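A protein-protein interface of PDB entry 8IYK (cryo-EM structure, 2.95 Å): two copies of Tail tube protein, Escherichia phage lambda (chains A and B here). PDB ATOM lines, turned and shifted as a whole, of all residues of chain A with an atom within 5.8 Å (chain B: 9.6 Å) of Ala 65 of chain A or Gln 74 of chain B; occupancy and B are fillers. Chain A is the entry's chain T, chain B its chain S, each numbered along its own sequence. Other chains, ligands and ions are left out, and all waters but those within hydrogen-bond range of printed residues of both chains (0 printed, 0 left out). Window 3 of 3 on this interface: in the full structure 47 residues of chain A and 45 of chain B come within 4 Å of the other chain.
NE2 of Gln 74 of chain B lies within hydrogen-bond range of O of Ala 65 of chain A, at 3.1 Å. O of Asp 66 of chain A is in hydrogen-bond range of N of Lys 75 of chain B (3.0 Å). The backbone NH (N) of Gly 147 of chain B sits at hydrogen-bond distance from the backbone carbonyl oxygen (O) of Thr 68 of chain A, at 3.2 Å.
N of Thr 51 of chain B sits close to O of Lys 75 of chain B, 3.5 Å away. The side-chain carboxylate of Asp 64 of chain A sits close to the side-chain carboxylate of Asp 66 of chain A, 2.7 Å away. O of Gln 74 of chain B is in hydrogen-bond range of N of Glu 53 of chain B (2.7 Å).
Among the printed residues, pairs that only touch across the chains: Thr 68 of chain A with Ser 76 of chain B (3.2 Å), Thr 68 of chain A with Gln 74 of chain B (3.2 Å), Trp 67 of chain A with Ala 77 of chain B (3.5 Å), Trp 67 of chain A with Lys 75 of chain B (3.5 Å), Asp 66 of chain A with Gln 74 of chain B (3.5 Å), Trp 67 of chain A with Arg 148 of chain B (3.6 Å), Trp 67 of chain A with Gln 74 of chain B (3.6 Å), Trp 67 of chain A with Ser 76 of chain B (3.6 Å) and Trp 67 of chain A with Gly 147 of chain B (3.7 Å).
No residue of chain B comes within 4 Å of Asp 64 of chain A. Ala 65 of chain A touches just one residue of chain B: Gln 74. Of chain B, only Gln 74 (3.5 Å) and Lys 75 (3.0 Å) come within 4 Å of Asp 66 of chain A. Of the printed residues of chain B, Thr 68 of chain A touches Gln 74, Ser 76 and Gly 147. Thr 51 of chain B touches none of the printed residues of chain A. Glu 53 of chain B touches none of the printed residues of chain A. Gln 74 of chain B touches just these residues of chain A: Ala 65 (3.1 Å), Asp 66 (3.5 Å), Trp 67 (3.6 Å) and Thr 68 (3.2 Å). Of the printed residues of chain A, Lys 75 of chain B touches Asp 66 (3.0 Å) and Trp 67 (3.5 Å). Of the printed residues of chain A, Ser 76 of chain B touches Trp 67 and Thr 68. Of the printed residues of chain A, Arg 148 of chain B touches Trp 67. The nearest printed residue of chain B that does not touch Thr 68 of chain A is Glu 53 of chain B (4.2 Å).
Hydrophobic or aromatic side chains of chain B within 4 Å of the printed part of chain A: Ala 77. Of the 8 printed residues of chain A, 4 touch a printed residue of chain B. Printed residues of chain A that touch a printed residue of chain B: Ala 65, Asp 66, Trp 67 and Thr 68. Hydrophobic or aromatic side chains of chain A that line the printed part of chain B: Trp 67. Among the printed residues, 12 pairs touch across the chains. Among the printed residues, no Asp or Glu carboxylate lies within 4 Å of a Lys or Arg side-chain nitrogen of the other chain.
No position is printed for both chains. Of the 12 pairs that touch across the chains among the printed residues, none has its exchanged pair printed and touching as well.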
ATOM      1  N   ASP A  62     -11.902 -10.749  -8.015  1.00  0.00           N
ATOM      2  CA  ASP A  62     -12.649  -9.500  -8.002  1.00  0.00           C
ATOM      3  C   ASP A  62     -13.069  -9.129  -9.417  1.00  0.00           C
ATOM      4  O   ASP A  62     -12.229  -9.023 -10.315  1.00  0.00           O
ATOM      5  CB  ASP A  62     -11.804  -8.381  -7.398  1.00  0.00           C
ATOM      6  CG  ASP A  62     -12.120  -8.132  -5.940  1.00  0.00           C
ATOM      7  OD1 ASP A  62     -13.191  -8.577  -5.476  1.00  0.00           O
ATOM      8  OD2 ASP A  62     -11.299  -7.486  -5.259  1.00  0.00           O
ATOM      9  N   GLU A  63     -14.338  -8.861  -9.625  1.00  0.00           N
ATOM     10  CA  GLU A  63     -14.829  -8.467 -10.964  1.00  0.00           C
ATOM     11  C   GLU A  63     -13.931  -7.385 -11.561  1.00  0.00           C
ATOM     12  O   GLU A  63     -13.194  -7.706 -12.496  1.00  0.00           O
ATOM     13  CB  GLU A  63     -16.272  -7.989 -10.849  1.00  0.00           C
ATOM     14  CG  GLU A  63     -16.509  -6.966  -9.751  1.00  0.00           C
ATOM     15  CD  GLU A  63     -16.359  -7.457  -8.321  1.00  0.00           C
ATOM     16  OE1 GLU A  63     -15.941  -6.656  -7.465  1.00  0.00           O
ATOM     17  OE2 GLU A  63     -16.648  -8.642  -8.068  1.00  0.00           O
ATOM     18  N   ASP A  64     -13.993  -6.154 -11.051  1.00  0.00           N
ATOM     19  CA  ASP A  64     -13.259  -5.012 -11.651  1.00  0.00           C
ATOM     20  C   ASP A  64     -11.899  -4.814 -10.987  1.00  0.00           C
ATOM     21  O   ASP A  64     -11.853  -4.791  -9.754  1.00  0.00           O
ATOM     22  CB  ASP A  64     -14.063  -3.728 -11.478  1.00  0.00           C
ATOM     23  CG  ASP A  64     -13.233  -2.453 -11.531  1.00  0.00           C
ATOM     24  OD1 ASP A  64     -12.634  -2.096 -10.498  1.00  0.00           O
ATOM     25  OD2 ASP A  64     -13.207  -1.811 -12.598  1.00  0.00           O
ATOM     26  N   ALA A  65     -10.859  -4.587 -11.786  1.00  0.00           N
ATOM     27  CA  ALA A  65      -9.515  -4.365 -11.230  1.00  0.00           C
ATOM     28  C   ALA A  65      -8.801  -3.215 -11.937  1.00  0.00           C
ATOM     29  O   ALA A  65      -7.636  -3.018 -11.637  1.00  0.00           O
ATOM     30  CB  ALA A  65      -8.735  -5.622 -11.348  1.00  0.00           C
ATOM     31  N   ASP A  66      -9.469  -2.472 -12.800  1.00  0.00           N
ATOM     32  CA  ASP A  66      -8.846  -1.316 -13.429  1.00  0.00           C
ATOM     33  C   ASP A  66      -8.423  -0.259 -12.418  1.00  0.00           C
ATOM     34  O   ASP A  66      -7.555   0.563 -12.729  1.00  0.00           O
ATOM     35  CB  ASP A  66      -9.799  -0.705 -14.456  1.00  0.00           C
ATOM     36  CG  ASP A  66     -10.556  -1.756 -15.244  1.00  0.00           C
ATOM     37  OD1 ASP A  66     -11.534  -2.314 -14.706  1.00  0.00           O
ATOM     38  OD2 ASP A  66     -10.171  -2.025 -16.401  1.00  0.00           O
ATOM     39  N   TRP A  67      -9.009  -0.261 -11.224  1.00  0.00           N
ATOM     40  CA  TRP A  67      -8.656   0.680 -10.174  1.00  0.00           C
ATOM     41  C   TRP A  67      -8.259  -0.093  -8.925  1.00  0.00           C
ATOM     42  O   TRP A  67      -8.535  -1.288  -8.796  1.00  0.00           O
ATOM     43  CB  TRP A  67      -9.817   1.635  -9.862  1.00  0.00           C
ATOM     44  CG  TRP A  67     -10.230   2.463 -11.036  1.00  0.00           C
ATOM     45  CD1 TRP A  67     -10.988   2.059 -12.092  1.00  0.00           C
ATOM     46  CD2 TRP A  67      -9.901   3.835 -11.280  1.00  0.00           C
ATOM     47  NE1 TRP A  67     -11.156   3.094 -12.978  1.00  0.00           N
ATOM     48  CE2 TRP A  67     -10.497   4.196 -12.502  1.00  0.00           C
ATOM     49  CE3 TRP A  67      -9.161   4.793 -10.582  1.00  0.00           C
ATOM     50  CZ2 TRP A  67     -10.378   5.473 -13.042  1.00  0.00           C
ATOM     51  CZ3 TRP A  67      -9.043   6.059 -11.121  1.00  0.00           C
ATOM     52  CH2 TRP A  67      -9.648   6.388 -12.337  1.00  0.00           C
ATOM     53  N   THR A  68      -7.603   0.601  -8.001  1.00  0.00           N
ATOM     54  CA  THR A  68      -7.123  -0.023  -6.776  1.00  0.00           C
ATOM     55  C   THR A  68      -8.153   0.116  -5.664  1.00  0.00           C
ATOM     56  O   THR A  68      -8.753   1.178  -5.482  1.00  0.00           O
ATOM     57  CB  THR A  68      -5.801   0.598  -6.325  1.00  0.00           C
ATOM     58  OG1 THR A  68      -5.979   2.004  -6.120  1.00  0.00           O
ATOM     59  CG2 THR A  68      -4.728   0.370  -7.367  1.00  0.00           C
ATOM     60  N   ALA A  69      -8.348  -0.969  -4.923  1.00  0.00           N
ATOM     61  CA  ALA A  69      -9.215  -0.985  -3.753  1.00  0.00           C
ATOM     62  C   ALA A  69      -8.340  -1.085  -2.514  1.00  0.00           C
ATOM     63  O   ALA A  69      -7.551  -2.027  -2.382  1.00  0.00           O
ATOM     64  CB  ALA A  69     -10.203  -2.149  -3.813  1.00  0.00           C
ATOM     65  N   GLU B  49      -4.932  13.249  -7.872  1.00  0.00           N
ATOM     66  CA  GLU B  49      -4.394  13.140  -9.221  1.00  0.00           C
ATOM     67  C   GLU B  49      -4.554  11.698  -9.676  1.00  0.00           C
ATOM     68  O   GLU B  49      -3.898  10.797  -9.142  1.00  0.00           O
ATOM     69  CB  GLU B  49      -2.931  13.571  -9.256  1.00  0.00           C
ATOM     70  CG  GLU B  49      -2.281  13.449 -10.617  1.00  0.00           C
ATOM     71  CD  GLU B  49      -0.823  13.057 -10.523  1.00  0.00           C
ATOM     72  OE1 GLU B  49      -0.263  13.129  -9.410  1.00  0.00           O
ATOM     73  OE2 GLU B  49      -0.237  12.679 -11.557  1.00  0.00           O
ATOM     74  N   LEU B  50      -5.428  11.477 -10.652  1.00  0.00           N
ATOM     75  CA  LEU B  50      -5.620  10.137 -11.186  1.00  0.00           C
ATOM     76  C   LEU B  50      -4.357   9.702 -11.916  1.00  0.00           C
ATOM     77  O   LEU B  50      -3.831  10.435 -12.756  1.00  0.00           O
ATOM     78  CB  LEU B  50      -6.819  10.099 -12.130  1.00  0.00           C
ATOM     79  CG  LEU B  50      -8.006  11.026 -11.858  1.00  0.00           C
ATOM     80  CD1 LEU B  50      -9.088  10.796 -12.894  1.00  0.00           C
ATOM     81  CD2 LEU B  50      -8.561  10.834 -10.464  1.00  0.00           C
ATOM     82  N   THR B  51      -3.877   8.508 -11.600  1.00  0.00           N
ATOM     83  CA  THR B  51      -2.620   8.003 -12.130  1.00  0.00           C
ATOM     84  C   THR B  51      -2.910   6.741 -12.944  1.00  0.00           C
ATOM     85  O   THR B  51      -4.067   6.391 -13.190  1.00  0.00           O
ATOM     86  CB  THR B  51      -1.634   7.755 -10.984  1.00  0.00           C
ATOM     87  OG1 THR B  51      -1.808   8.768  -9.988  1.00  0.00           O
ATOM     88  CG2 THR B  51      -0.198   7.835 -11.478  1.00  0.00           C
ATOM     89  N   ALA B  52      -1.847   6.068 -13.384  1.00  0.00           N
ATOM     90  CA  ALA B  52      -1.969   4.798 -14.085  1.00  0.00           C
ATOM     91  C   ALA B  52      -0.610   4.120 -14.094  1.00  0.00           C
ATOM     92  O   ALA B  52       0.378   4.723 -14.519  1.00  0.00           O
ATOM     93  CB  ALA B  52      -2.476   4.997 -15.516  1.00  0.00           C
ATOM     94  N   GLU B  53      -0.562   2.875 -13.630  1.00  0.00           N
ATOM     95  CA  GLU B  53       0.683   2.131 -13.675  1.00  0.00           C
ATOM     96  C   GLU B  53       0.976   1.667 -15.098  1.00  0.00           C
ATOM     97  O   GLU B  53       0.080   1.520 -15.932  1.00  0.00           O
ATOM     98  CB  GLU B  53       0.638   0.927 -12.735  1.00  0.00           C
ATOM     99  CG  GLU B  53       0.290   1.264 -11.300  1.00  0.00           C
ATOM    100  CD  GLU B  53      -0.315   0.091 -10.560  1.00  0.00           C
ATOM    101  OE1 GLU B  53       0.052  -1.062 -10.873  1.00  0.00           O
ATOM    102  OE2 GLU B  53      -1.153   0.320  -9.662  1.00  0.00           O
ATOM    103  N   SER B  54       2.254   1.435 -15.367  1.00  0.00           N
ATOM    104  CA  SER B  54       2.713   1.002 -16.678  1.00  0.00           C
ATOM    105  C   SER B  54       2.883  -0.509 -16.683  1.00  0.00           C
ATOM    106  O   SER B  54       3.523  -1.069 -15.788  1.00  0.00           O
ATOM    107  CB  SER B  54       4.032   1.687 -17.040  1.00  0.00           C
ATOM    108  OG  SER B  54       4.778   0.903 -17.951  1.00  0.00           O
ATOM    109  N   TYR B  55       2.311  -1.163 -17.688  1.00  0.00           N
ATOM    110  CA  TYR B  55       2.424  -2.604 -17.859  1.00  0.00           C
ATOM    111  C   TYR B  55       3.346  -2.894 -19.032  1.00  0.00           C
ATOM    112  O   TYR B  55       3.172  -2.330 -20.118  1.00  0.00           O
ATOM    113  CB  TYR B  55       1.055  -3.243 -18.092  1.00  0.00           C
ATOM    114  CG  TYR B  55       1.125  -4.723 -18.380  1.00  0.00           C
ATOM    115  CD1 TYR B  55       1.553  -5.617 -17.409  1.00  0.00           C
ATOM    116  CD2 TYR B  55       0.774  -5.225 -19.624  1.00  0.00           C
ATOM    117  CE1 TYR B  55       1.622  -6.971 -17.667  1.00  0.00           C
ATOM    118  CE2 TYR B  55       0.839  -6.578 -19.890  1.00  0.00           C
ATOM    119  CZ  TYR B  55       1.263  -7.446 -18.909  1.00  0.00           C
ATOM    120  OH  TYR B  55       1.332  -8.794 -19.170  1.00  0.00           O
ATOM    121  N   GLY B  71       1.843  -0.415 -21.881  1.00  0.00           N
ATOM    122  CA  GLY B  71       0.411  -0.199 -21.894  1.00  0.00           C
ATOM    123  C   GLY B  71      -0.055   0.298 -20.544  1.00  0.00           C
ATOM    124  O   GLY B  71       0.699   0.314 -19.570  1.00  0.00           O
ATOM    125  N   GLN B  72      -1.316   0.713 -20.497  1.00  0.00           N
ATOM    126  CA  GLN B  72      -1.883   1.207 -19.252  1.00  0.00           C
ATOM    127  C   GLN B  72      -2.190   0.057 -18.300  1.00  0.00           C
ATOM    128  O   GLN B  72      -2.541  -1.050 -18.715  1.00  0.00           O
ATOM    129  CB  GLN B  72      -3.152   2.011 -19.524  1.00  0.00           C
ATOM    130  CG  GLN B  72      -3.344   3.174 -18.572  1.00  0.00           C
ATOM    131  CD  GLN B  72      -4.740   3.753 -18.635  1.00  0.00           C
ATOM    132  OE1 GLN B  72      -5.728   3.033 -18.504  1.00  0.00           O
ATOM    133  NE2 GLN B  72      -4.829   5.061 -18.832  1.00  0.00           N
ATOM    134  N   GLY B  73      -2.054   0.333 -17.006  1.00  0.00           N
ATOM    135  CA  GLY B  73      -2.361  -0.647 -15.985  1.00  0.00           C
ATOM    136  C   GLY B  73      -3.393  -0.152 -14.994  1.00  0.00           C
ATOM    137  O   GLY B  73      -4.355   0.521 -15.375  1.00  0.00           O
ATOM    138  N   GLN B  74      -3.209  -0.486 -13.720  1.00  0.00           N
ATOM    139  CA  GLN B  74      -4.117  -0.020 -12.681  1.00  0.00           C
ATOM    140  C   GLN B  74      -3.994   1.490 -12.508  1.00  0.00           C
ATOM    141  O   GLN B  74      -2.923   2.072 -12.689  1.00  0.00           O
ATOM    142  CB  GLN B  74      -3.820  -0.738 -11.366  1.00  0.00           C
ATOM    143  CG  GLN B  74      -5.047  -1.303 -10.682  1.00  0.00           C
ATOM    144  CD  GLN B  74      -4.693  -2.281  -9.586  1.00  0.00           C
ATOM    145  OE1 GLN B  74      -3.638  -2.174  -8.960  1.00  0.00           O
ATOM    146  NE2 GLN B  74      -5.572  -3.244  -9.346  1.00  0.00           N
ATOM    147  N   LYS B  75      -5.110   2.127 -12.147  1.00  0.00           N
ATOM    148  CA  LYS B  75      -5.222   3.582 -12.210  1.00  0.00           C
ATOM    149  C   LYS B  75      -4.982   4.255 -10.861  1.00  0.00           C
ATOM    150  O   LYS B  75      -4.115   5.126 -10.751  1.00  0.00           O
ATOM    151  CB  LYS B  75      -6.594   3.955 -12.779  1.00  0.00           C
ATOM    152  CG  LYS B  75      -6.790   3.485 -14.209  1.00  0.00           C
ATOM    153  CD  LYS B  75      -7.565   4.491 -15.029  1.00  0.00           C
ATOM    154  CE  LYS B  75      -8.020   3.888 -16.342  1.00  0.00           C
ATOM    155  NZ  LYS B  75      -8.902   2.710 -16.140  1.00  0.00           N
ATOM    156  N   SER B  76      -5.733   3.871  -9.828  1.00  0.00           N
ATOM    157  CA  SER B  76      -5.470   4.284  -8.447  1.00  0.00           C
ATOM    158  C   SER B  76      -5.550   5.806  -8.269  1.00  0.00           C
ATOM    159  O   SER B  76      -4.561   6.483  -7.981  1.00  0.00           O
ATOM    160  CB  SER B  76      -4.103   3.766  -7.983  1.00  0.00           C
ATOM    161  OG  SER B  76      -3.115   4.775  -8.099  1.00  0.00           O
ATOM    162  N   ALA B  77      -6.758   6.331  -8.455  1.00  0.00           N
ATOM    163  CA  ALA B  77      -7.060   7.678  -7.980  1.00  0.00           C
ATOM    164  C   ALA B  77      -6.853   7.750  -6.473  1.00  0.00           C
ATOM    165  O   ALA B  77      -7.290   6.860  -5.740  1.00  0.00           O
ATOM    166  CB  ALA B  77      -8.497   8.052  -8.327  1.00  0.00           C
ATOM    167  N   GLY B 147     -11.259   3.212  -5.605  1.00  0.00           N
ATOM    168  CA  GLY B 147     -12.180   2.979  -6.691  1.00  0.00           C
ATOM    169  C   GLY B 147     -12.196   4.090  -7.729  1.00  0.00           C
ATOM    170  O   GLY B 147     -11.418   5.043  -7.700  1.00  0.00           O
ATOM    171  N   ARG B 148     -13.126   3.940  -8.661  1.00  0.00           N
ATOM    172  CA  ARG B 148     -13.295   4.890  -9.751  1.00  0.00           C
ATOM    173  C   ARG B 148     -14.061   6.116  -9.266  1.00  0.00           C
ATOM    174  O   ARG B 148     -15.171   5.978  -8.744  1.00  0.00           O
ATOM    175  CB  ARG B 148     -14.042   4.237 -10.907  1.00  0.00           C
ATOM    176  CG  ARG B 148     -14.063   5.048 -12.185  1.00  0.00           C
ATOM    177  CD  ARG B 148     -15.319   4.751 -12.982  1.00  0.00           C
ATOM    178  NE  ARG B 148     -15.709   5.874 -13.825  1.00  0.00           N
ATOM    179  CZ  ARG B 148     -15.648   5.871 -15.149  1.00  0.00           C
ATOM    180  NH1 ARG B 148     -15.220   4.814 -15.818  1.00  0.00           N
ATOM    181  NH2 ARG B 148     -16.033   6.955 -15.817  1.00  0.00           N
